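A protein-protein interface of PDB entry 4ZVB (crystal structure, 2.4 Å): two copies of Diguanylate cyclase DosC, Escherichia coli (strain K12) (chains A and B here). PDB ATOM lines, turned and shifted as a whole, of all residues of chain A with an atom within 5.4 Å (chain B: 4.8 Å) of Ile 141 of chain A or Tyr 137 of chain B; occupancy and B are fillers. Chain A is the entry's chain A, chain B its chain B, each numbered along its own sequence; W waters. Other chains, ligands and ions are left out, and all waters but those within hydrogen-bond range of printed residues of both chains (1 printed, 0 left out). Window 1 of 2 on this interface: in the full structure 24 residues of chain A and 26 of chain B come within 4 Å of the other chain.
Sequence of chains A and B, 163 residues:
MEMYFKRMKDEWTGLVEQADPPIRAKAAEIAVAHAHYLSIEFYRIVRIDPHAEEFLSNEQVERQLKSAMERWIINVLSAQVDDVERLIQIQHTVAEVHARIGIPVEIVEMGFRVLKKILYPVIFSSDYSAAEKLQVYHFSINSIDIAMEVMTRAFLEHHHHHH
ND1 of His 138 of chain B is in hydrogen-bond range of OH of Tyr 137 of chain A, at 3.4 Å.
The side-chain carboxylate (OD1) of Asp 145 of chain A is in salt-bridge range of the side-chain amino group (NZ) of Lys 116 of chain B, at 3.3 Å.
NZ of Lys 116 of chain B sits close to NZ of Lys 116 of chain A (3.3 Å).
The side-chain amino group of Lys 116 of chain A is in salt-bridge range of the side-chain carboxylate of Asp 145 of chain A (3.0 Å).
NE2 of His 138 of chain A is in hydrogen-bond range of ND2 of Asn 142 of chain A (3.1 Å).
Among the printed residues, pairs that only touch across the chains: Leu 134 of chain A with Tyr 120 of chain B (3.8 Å), Leu 134 of chain A with Lys 133 of chain B (3.9 Å), Leu 134 of chain A with Leu 134 of chain B (3.7 Å), Tyr 137 of chain A with Tyr 137 of chain B (3.4 Å), His 138 of chain A with Tyr 120 of chain B (3.3 Å), His 138 of chain A with Tyr 137 of chain B (3.6 Å), Ile 141 of chain A with Tyr 137 of chain B (3.96 Å) and Asn 142 of chain A with Tyr 137 of chain B (3.9 Å).
Of the printed residues of chain B, Tyr 137 of chain A touches Tyr 137 and His 138.
Ile 141 of chain A touches just one residue of chain B: Tyr 137 (3.96 Å).
Of the printed residues of chain A, Lys 116 of chain B touches Lys 116 (3.3 Å) and Asp 145 (3.3 Å).
Printed residues of chain A within 4 Å of Leu 134 of chain B: Leu 134.
Tyr 137 of chain B touches just these residues of chain A: Tyr 137, His 138, Ile 141 and Asn 142.
The nearest printed residue of chain A that does not touch Lys 133 of chain B is Tyr 137 of chain A (7.1 Å).
Of the 12 printed residues of chain B, 6 touch a printed residue of chain A.
Hydrophobic or aromatic side chains of chain B within 4 Å of the printed part of chain A: Tyr 120, Leu 134, Tyr 137 and His 138.
Among the printed residues, 11 pairs touch across the chains.
Lys 116 of chain A touches its own counterpart, Lys 116 of chain B.
Leu 134 of chain B touches its own counterpart, Leu 134 of chain A.
Tyr 137 of chain A touches His 138 of chain B, and with the chains exchanged His 138 of chain A touches Tyr 137 of chain B.
Ile 141 of chain A touches Tyr 137 of chain B, but with the chains exchanged Tyr 137 of chain A does not touch Ile 141 of chain B (4.1 Å).
Of the 11 pairs that touch across the chains among the printed residues, 5 have their exchanged pair printed and touching as well.
Water W1 lies within hydrogen-bond range of OH of Tyr 137 of chain B (2.4 Å), O of Lys 116 of chain B (2.6 Å) and OD1 of Asn 142 of chain A (2.8 Å).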
ATOM      1  N   LYS A 116     -22.468   9.852 -23.887  1.00  0.00           N
ATOM      2  CA  LYS A 116     -22.685   8.809 -24.884  1.00  0.00           C
ATOM      3  C   LYS A 116     -23.332   9.366 -26.149  1.00  0.00           C
ATOM      4  O   LYS A 116     -23.126   8.842 -27.244  1.00  0.00           O
ATOM      5  CB  LYS A 116     -23.545   7.684 -24.302  1.00  0.00           C
ATOM      6  CG  LYS A 116     -22.851   6.883 -23.210  1.00  0.00           C
ATOM      7  CD  LYS A 116     -23.735   5.762 -22.686  1.00  0.00           C
ATOM      8  CE  LYS A 116     -24.894   6.310 -21.867  1.00  0.00           C
ATOM      9  NZ  LYS A 116     -25.716   5.221 -21.267  1.00  0.00           N
ATOM     10  N   LEU A 134     -19.176   0.761 -36.067  1.00  0.00           N
ATOM     11  CA  LEU A 134     -20.146   0.027 -35.265  1.00  0.00           C
ATOM     12  C   LEU A 134     -19.486  -0.651 -34.070  1.00  0.00           C
ATOM     13  O   LEU A 134     -20.015  -0.624 -32.958  1.00  0.00           O
ATOM     14  CB  LEU A 134     -20.866  -1.014 -36.124  1.00  0.00           C
ATOM     15  CG  LEU A 134     -21.845  -1.940 -35.399  1.00  0.00           C
ATOM     16  CD1 LEU A 134     -22.961  -1.141 -34.744  1.00  0.00           C
ATOM     17  CD2 LEU A 134     -22.410  -2.976 -36.359  1.00  0.00           C
ATOM     18  N   VAL A 136     -16.419   0.064 -32.738  1.00  0.00           N
ATOM     19  CA  VAL A 136     -15.825   1.069 -31.862  1.00  0.00           C
ATOM     20  C   VAL A 136     -16.894   1.685 -30.963  1.00  0.00           C
ATOM     21  O   VAL A 136     -16.692   1.853 -29.759  1.00  0.00           O
ATOM     22  CB  VAL A 136     -15.118   2.179 -32.668  1.00  0.00           C
ATOM     23  CG1 VAL A 136     -14.828   3.386 -31.786  1.00  0.00           C
ATOM     24  CG2 VAL A 136     -13.832   1.647 -33.283  1.00  0.00           C
ATOM     25  N   TYR A 137     -18.036   2.010 -31.560  1.00  0.00           N
ATOM     26  CA  TYR A 137     -19.158   2.592 -30.833  1.00  0.00           C
ATOM     27  C   TYR A 137     -19.709   1.609 -29.804  1.00  0.00           C
ATOM     28  O   TYR A 137     -20.071   1.996 -28.694  1.00  0.00           O
ATOM     29  CB  TYR A 137     -20.253   3.024 -31.813  1.00  0.00           C
ATOM     30  CG  TYR A 137     -21.465   3.660 -31.174  1.00  0.00           C
ATOM     31  CD1 TYR A 137     -21.347   4.805 -30.397  1.00  0.00           C
ATOM     32  CD2 TYR A 137     -22.734   3.131 -31.371  1.00  0.00           C
ATOM     33  CE1 TYR A 137     -22.456   5.394 -29.819  1.00  0.00           C
ATOM     34  CE2 TYR A 137     -23.849   3.712 -30.798  1.00  0.00           C
ATOM     35  CZ  TYR A 137     -23.705   4.844 -30.024  1.00  0.00           C
ATOM     36  OH  TYR A 137     -24.813   5.424 -29.452  1.00  0.00           O
ATOM     37  N   HIS A 138     -19.761   0.335 -30.179  1.00  0.00           N
ATOM     38  CA  HIS A 138     -20.225  -0.715 -29.277  1.00  0.00           C
ATOM     39  C   HIS A 138     -19.308  -0.869 -28.069  1.00  0.00           C
ATOM     40  O   HIS A 138     -19.773  -0.965 -26.933  1.00  0.00           O
ATOM     41  CB  HIS A 138     -20.331  -2.047 -30.016  1.00  0.00           C
ATOM     42  CG  HIS A 138     -20.500  -3.227 -29.110  1.00  0.00           C
ATOM     43  ND1 HIS A 138     -19.569  -4.240 -29.026  1.00  0.00           N
ATOM     44  CD2 HIS A 138     -21.486  -3.548 -28.239  1.00  0.00           C
ATOM     45  CE1 HIS A 138     -19.978  -5.139 -28.148  1.00  0.00           C
ATOM     46  NE2 HIS A 138     -21.138  -4.743 -27.656  1.00  0.00           N
ATOM     47  N   PHE A 139     -18.004  -0.894 -28.325  1.00  0.00           N
ATOM     48  CA  PHE A 139     -17.015  -1.017 -27.262  1.00  0.00           C
ATOM     49  C   PHE A 139     -17.048   0.207 -26.351  1.00  0.00           C
ATOM     50  O   PHE A 139     -16.902   0.091 -25.136  1.00  0.00           O
ATOM     51  CB  PHE A 139     -15.615  -1.203 -27.853  1.00  0.00           C
ATOM     52  CG  PHE A 139     -14.510  -1.114 -26.839  1.00  0.00           C
ATOM     53  CD1 PHE A 139     -14.267  -2.163 -25.967  1.00  0.00           C
ATOM     54  CD2 PHE A 139     -13.714   0.017 -26.759  1.00  0.00           C
ATOM     55  CE1 PHE A 139     -13.251  -2.086 -25.033  1.00  0.00           C
ATOM     56  CE2 PHE A 139     -12.696   0.100 -25.827  1.00  0.00           C
ATOM     57  CZ  PHE A 139     -12.465  -0.953 -24.962  1.00  0.00           C
ATOM     58  N   SER A 140     -17.246   1.377 -26.951  1.00  0.00           N
ATOM     59  CA  SER A 140     -17.286   2.630 -26.204  1.00  0.00           C
ATOM     60  C   SER A 140     -18.502   2.703 -25.286  1.00  0.00           C
ATOM     61  O   SER A 140     -18.391   3.107 -24.130  1.00  0.00           O
ATOM     62  CB  SER A 140     -17.286   3.822 -27.164  1.00  0.00           C
ATOM     63  OG  SER A 140     -16.107   3.847 -27.948  1.00  0.00           O
ATOM     64  N   ILE A 141     -19.661   2.311 -25.807  1.00  0.00           N
ATOM     65  CA  ILE A 141     -20.899   2.341 -25.036  1.00  0.00           C
ATOM     66  C   ILE A 141     -20.836   1.386 -23.846  1.00  0.00           C
ATOM     67  O   ILE A 141     -21.173   1.760 -22.722  1.00  0.00           O
ATOM     68  CB  ILE A 141     -22.120   1.991 -25.912  1.00  0.00           C
ATOM     69  CG1 ILE A 141     -22.423   3.135 -26.880  1.00  0.00           C
ATOM     70  CG2 ILE A 141     -23.343   1.718 -25.052  1.00  0.00           C
ATOM     71  CD1 ILE A 141     -22.744   4.444 -26.188  1.00  0.00           C
ATOM     72  N   ASN A 142     -20.398   0.156 -24.096  1.00  0.00           N
ATOM     73  CA  ASN A 142     -20.301  -0.842 -23.036  1.00  0.00           C
ATOM     74  C   ASN A 142     -19.278  -0.463 -21.968  1.00  0.00           C
ATOM     75  O   ASN A 142     -19.482  -0.731 -20.786  1.00  0.00           O
ATOM     76  CB  ASN A 142     -19.955  -2.211 -23.626  1.00  0.00           C
ATOM     77  CG  ASN A 142     -21.125  -2.846 -24.352  1.00  0.00           C
ATOM     78  OD1 ASN A 142     -22.110  -2.179 -24.671  1.00  0.00           O
ATOM     79  ND2 ASN A 142     -21.025  -4.143 -24.616  1.00  0.00           N
ATOM     80  N   SER A 143     -18.184   0.162 -22.392  1.00  0.00           N
ATOM     81  CA  SER A 143     -17.145   0.605 -21.466  1.00  0.00           C
ATOM     82  C   SER A 143     -17.641   1.720 -20.549  1.00  0.00           C
ATOM     83  O   SER A 143     -17.360   1.723 -19.353  1.00  0.00           O
ATOM     84  CB  SER A 143     -15.908   1.075 -22.235  1.00  0.00           C
ATOM     85  OG  SER A 143     -15.321   0.009 -22.963  1.00  0.00           O
ATOM     86  N   ILE A 144     -18.372   2.670 -21.120  1.00  0.00           N
ATOM     87  CA  ILE A 144     -18.924   3.777 -20.349  1.00  0.00           C
ATOM     88  C   ILE A 144     -20.033   3.284 -19.419  1.00  0.00           C
ATOM     89  O   ILE A 144     -20.173   3.761 -18.292  1.00  0.00           O
ATOM     90  CB  ILE A 144     -19.463   4.889 -21.277  1.00  0.00           C
ATOM     91  CG1 ILE A 144     -18.316   5.505 -22.082  1.00  0.00           C
ATOM     92  CG2 ILE A 144     -20.169   5.972 -20.478  1.00  0.00           C
ATOM     93  CD1 ILE A 144     -18.766   6.515 -23.117  1.00  0.00           C
ATOM     94  N   ASP A 145     -20.805   2.310 -19.892  1.00  0.00           N
ATOM     95  CA  ASP A 145     -21.909   1.758 -19.114  1.00  0.00           C
ATOM     96  C   ASP A 145     -21.424   0.995 -17.883  1.00  0.00           C
ATOM     97  O   ASP A 145     -21.964   1.168 -16.791  1.00  0.00           O
ATOM     98  CB  ASP A 145     -22.773   0.844 -19.985  1.00  0.00           C
ATOM     99  CG  ASP A 145     -23.711   1.619 -20.891  1.00  0.00           C
ATOM    100  OD1 ASP A 145     -24.046   2.774 -20.552  1.00  0.00           O
ATOM    101  OD2 ASP A 145     -24.113   1.075 -21.941  1.00  0.00           O
ATOM    102  N   ILE A 146     -20.412   0.150 -18.060  1.00  0.00           N
ATOM    103  CA  ILE A 146     -19.877  -0.623 -16.942  1.00  0.00           C
ATOM    104  C   ILE A 146     -19.184   0.310 -15.948  1.00  0.00           C
ATOM    105  O   ILE A 146     -19.218   0.076 -14.742  1.00  0.00           O
ATOM    106  CB  ILE A 146     -18.901  -1.736 -17.417  1.00  0.00           C
ATOM    107  CG1 ILE A 146     -18.448  -2.601 -16.238  1.00  0.00           C
ATOM    108  CG2 ILE A 146     -17.697  -1.155 -18.137  1.00  0.00           C
ATOM    109  CD1 ILE A 146     -19.570  -3.348 -15.558  1.00  0.00           C
ATOM    110  N   LYS B 116     -29.037  -3.349 -23.094  1.00  0.00           N
ATOM    111  CA  LYS B 116     -28.292  -2.683 -24.155  1.00  0.00           C
ATOM    112  C   LYS B 116     -27.135  -3.551 -24.638  1.00  0.00           C
ATOM    113  O   LYS B 116     -26.733  -3.482 -25.799  1.00  0.00           O
ATOM    114  CB  LYS B 116     -27.768  -1.329 -23.673  1.00  0.00           C
ATOM    115  CG  LYS B 116     -28.861  -0.303 -23.416  1.00  0.00           C
ATOM    116  CD  LYS B 116     -28.289   1.033 -22.965  1.00  0.00           C
ATOM    117  CE  LYS B 116     -27.727   0.950 -21.558  1.00  0.00           C
ATOM    118  NZ  LYS B 116     -27.252   2.275 -21.072  1.00  0.00           N
ATOM    119  N   TYR B 120     -27.021  -5.745 -28.889  1.00  0.00           N
ATOM    120  CA  TYR B 120     -26.011  -5.590 -29.933  1.00  0.00           C
ATOM    121  C   TYR B 120     -25.774  -6.842 -30.797  1.00  0.00           C
ATOM    122  O   TYR B 120     -25.708  -6.725 -32.020  1.00  0.00           O
ATOM    123  CB  TYR B 120     -24.686  -5.136 -29.313  1.00  0.00           C
ATOM    124  CG  TYR B 120     -23.552  -5.019 -30.307  1.00  0.00           C
ATOM    125  CD1 TYR B 120     -23.484  -3.946 -31.188  1.00  0.00           C
ATOM    126  CD2 TYR B 120     -22.546  -5.975 -30.361  1.00  0.00           C
ATOM    127  CE1 TYR B 120     -22.451  -3.833 -32.098  1.00  0.00           C
ATOM    128  CE2 TYR B 120     -21.507  -5.868 -31.267  1.00  0.00           C
ATOM    129  CZ  TYR B 120     -21.464  -4.795 -32.132  1.00  0.00           C
ATOM    130  OH  TYR B 120     -20.433  -4.683 -33.036  1.00  0.00           O
ATOM    131  N   ILE B 123     -28.634  -7.195 -33.338  1.00  0.00           N
ATOM    132  CA  ILE B 123     -28.547  -6.236 -34.432  1.00  0.00           C
ATOM    133  C   ILE B 123     -27.374  -6.573 -35.352  1.00  0.00           C
ATOM    134  O   ILE B 123     -27.470  -6.445 -36.573  1.00  0.00           O
ATOM    135  CB  ILE B 123     -28.391  -4.794 -33.907  1.00  0.00           C
ATOM    136  CG1 ILE B 123     -29.571  -4.425 -33.004  1.00  0.00           C
ATOM    137  CG2 ILE B 123     -28.275  -3.806 -35.061  1.00  0.00           C
ATOM    138  CD1 ILE B 123     -29.519  -3.006 -32.478  1.00  0.00           C
ATOM    139  N   LYS B 133     -26.891  -1.010 -39.580  1.00  0.00           N
ATOM    140  CA  LYS B 133     -26.716  -1.577 -38.246  1.00  0.00           C
ATOM    141  C   LYS B 133     -26.222  -0.530 -37.255  1.00  0.00           C
ATOM    142  O   LYS B 133     -26.621  -0.528 -36.092  1.00  0.00           O
ATOM    143  CB  LYS B 133     -25.746  -2.759 -38.284  1.00  0.00           C
ATOM    144  CG  LYS B 133     -26.313  -4.011 -38.929  1.00  0.00           C
ATOM    145  CD  LYS B 133     -25.258  -5.099 -39.036  1.00  0.00           C
ATOM    146  CE  LYS B 133     -25.826  -6.357 -39.669  1.00  0.00           C
ATOM    147  NZ  LYS B 133     -24.788  -7.410 -39.851  1.00  0.00           N
ATOM    148  N   LEU B 134     -25.351   0.358 -37.726  1.00  0.00           N
ATOM    149  CA  LEU B 134     -24.797   1.414 -36.889  1.00  0.00           C
ATOM    150  C   LEU B 134     -25.880   2.386 -36.429  1.00  0.00           C
ATOM    151  O   LEU B 134     -25.918   2.783 -35.264  1.00  0.00           O
ATOM    152  CB  LEU B 134     -23.699   2.169 -37.644  1.00  0.00           C
ATOM    153  CG  LEU B 134     -23.077   3.381 -36.949  1.00  0.00           C
ATOM    154  CD1 LEU B 134     -22.418   2.977 -35.638  1.00  0.00           C
ATOM    155  CD2 LEU B 134     -22.076   4.068 -37.867  1.00  0.00           C
ATOM    156  N   GLN B 135     -26.762   2.760 -37.350  1.00  0.00           N
ATOM    157  CA  GLN B 135     -27.826   3.713 -37.053  1.00  0.00           C
ATOM    158  C   GLN B 135     -28.947   3.075 -36.233  1.00  0.00           C
ATOM    159  O   GLN B 135     -29.535   3.722 -35.367  1.00  0.00           O
ATOM    160  CB  GLN B 135     -28.382   4.307 -38.348  1.00  0.00           C
ATOM    161  CG  GLN B 135     -27.337   5.041 -39.172  1.00  0.00           C
ATOM    162  CD  GLN B 135     -27.902   5.628 -40.448  1.00  0.00           C
ATOM    163  OE1 GLN B 135     -28.912   6.331 -40.429  1.00  0.00           O
ATOM    164  NE2 GLN B 135     -27.250   5.344 -41.569  1.00  0.00           N
ATOM    165  N   VAL B 136     -29.240   1.807 -36.511  1.00  0.00           N
ATOM    166  CA  VAL B 136     -30.233   1.066 -35.739  1.00  0.00           C
ATOM    167  C   VAL B 136     -29.770   0.914 -34.295  1.00  0.00           C
ATOM    168  O   VAL B 136     -30.544   1.121 -33.357  1.00  0.00           O
ATOM    169  CB  VAL B 136     -30.503  -0.329 -36.348  1.00  0.00           C
ATOM    170  CG1 VAL B 136     -31.219  -1.228 -35.348  1.00  0.00           C
ATOM    171  CG2 VAL B 136     -31.307  -0.205 -37.634  1.00  0.00           C
ATOM    172  N   TYR B 137     -28.500   0.562 -34.126  1.00  0.00           N
ATOM    173  CA  TYR B 137     -27.912   0.412 -32.801  1.00  0.00           C
ATOM    174  C   TYR B 137     -27.881   1.750 -32.068  1.00  0.00           C
ATOM    175  O   TYR B 137     -28.130   1.815 -30.865  1.00  0.00           O
ATOM    176  CB  TYR B 137     -26.502  -0.172 -32.907  1.00  0.00           C
ATOM    177  CG  TYR B 137     -25.808  -0.377 -31.581  1.00  0.00           C
ATOM    178  CD1 TYR B 137     -26.354  -1.206 -30.609  1.00  0.00           C
ATOM    179  CD2 TYR B 137     -24.603   0.252 -31.305  1.00  0.00           C
ATOM    180  CE1 TYR B 137     -25.717  -1.398 -29.395  1.00  0.00           C
ATOM    181  CE2 TYR B 137     -23.960   0.067 -30.096  1.00  0.00           C
ATOM    182  CZ  TYR B 137     -24.520  -0.759 -29.145  1.00  0.00           C
ATOM    183  OH  TYR B 137     -23.881  -0.943 -27.941  1.00  0.00           O
ATOM    184  N   HIS B 138     -27.582   2.815 -32.806  1.00  0.00           N
ATOM    185  CA  HIS B 138     -27.550   4.158 -32.237  1.00  0.00           C
ATOM    186  C   HIS B 138     -28.924   4.594 -31.740  1.00  0.00           C
ATOM    187  O   HIS B 138     -29.055   5.125 -30.636  1.00  0.00           O
ATOM    188  CB  HIS B 138     -27.032   5.164 -33.264  1.00  0.00           C
ATOM    189  CG  HIS B 138     -27.250   6.595 -32.869  1.00  0.00           C
ATOM    190  ND1 HIS B 138     -26.583   7.183 -31.822  1.00  0.00           N
ATOM    191  CD2 HIS B 138     -28.072   7.539 -33.381  1.00  0.00           C
ATOM    192  CE1 HIS B 138     -26.981   8.443 -31.705  1.00  0.00           C
ATOM    193  NE2 HIS B 138     -27.880   8.682 -32.636  1.00  0.00           N
ATOM    194  N   PHE B 139     -29.943   4.373 -32.566  1.00  0.00           N
ATOM    195  CA  PHE B 139     -31.311   4.715 -32.200  1.00  0.00           C
ATOM    196  C   PHE B 139     -31.799   3.876 -31.027  1.00  0.00           C
ATOM    197  O   PHE B 139     -32.506   4.372 -30.151  1.00  0.00           O
ATOM    198  CB  PHE B 139     -32.251   4.539 -33.396  1.00  0.00           C
ATOM    199  CG  PHE B 139     -33.707   4.626 -33.036  1.00  0.00           C
ATOM    200  CD1 PHE B 139     -34.293   5.849 -32.753  1.00  0.00           C
ATOM    201  CD2 PHE B 139     -34.490   3.486 -32.985  1.00  0.00           C
ATOM    202  CE1 PHE B 139     -35.631   5.930 -32.421  1.00  0.00           C
ATOM    203  CE2 PHE B 139     -35.829   3.562 -32.654  1.00  0.00           C
ATOM    204  CZ  PHE B 139     -36.401   4.785 -32.372  1.00  0.00           C
ATOM    205  N   SER B 140     -31.414   2.604 -31.017  1.00  0.00           N
ATOM    206  CA  SER B 140     -31.828   1.689 -29.959  1.00  0.00           C
ATOM    207  C   SER B 140     -31.218   2.075 -28.616  1.00  0.00           C
ATOM    208  O   SER B 140     -31.906   2.084 -27.598  1.00  0.00           O
ATOM    209  CB  SER B 140     -31.445   0.252 -30.315  1.00  0.00           C
ATOM    210  OG  SER B 140     -32.096  -0.172 -31.501  1.00  0.00           O
ATOM    211  N   ILE B 141     -29.928   2.400 -28.621  1.00  0.00           N
ATOM    212  CA  ILE B 141     -29.230   2.776 -27.396  1.00  0.00           C
ATOM    213  C   ILE B 141     -29.803   4.062 -26.806  1.00  0.00           C
ATOM    214  O   ILE B 141     -30.088   4.133 -25.610  1.00  0.00           O
ATOM    215  CB  ILE B 141     -27.715   2.955 -27.639  1.00  0.00           C
ATOM    216  CG1 ILE B 141     -27.054   1.599 -27.890  1.00  0.00           C
ATOM    217  CG2 ILE B 141     -27.054   3.638 -26.452  1.00  0.00           C
ATOM    218  CD1 ILE B 141     -27.195   0.632 -26.738  1.00  0.00           C
HETATM  219  O   HOH W   1     -24.341  -2.653 -26.305  1.00  0.00           O
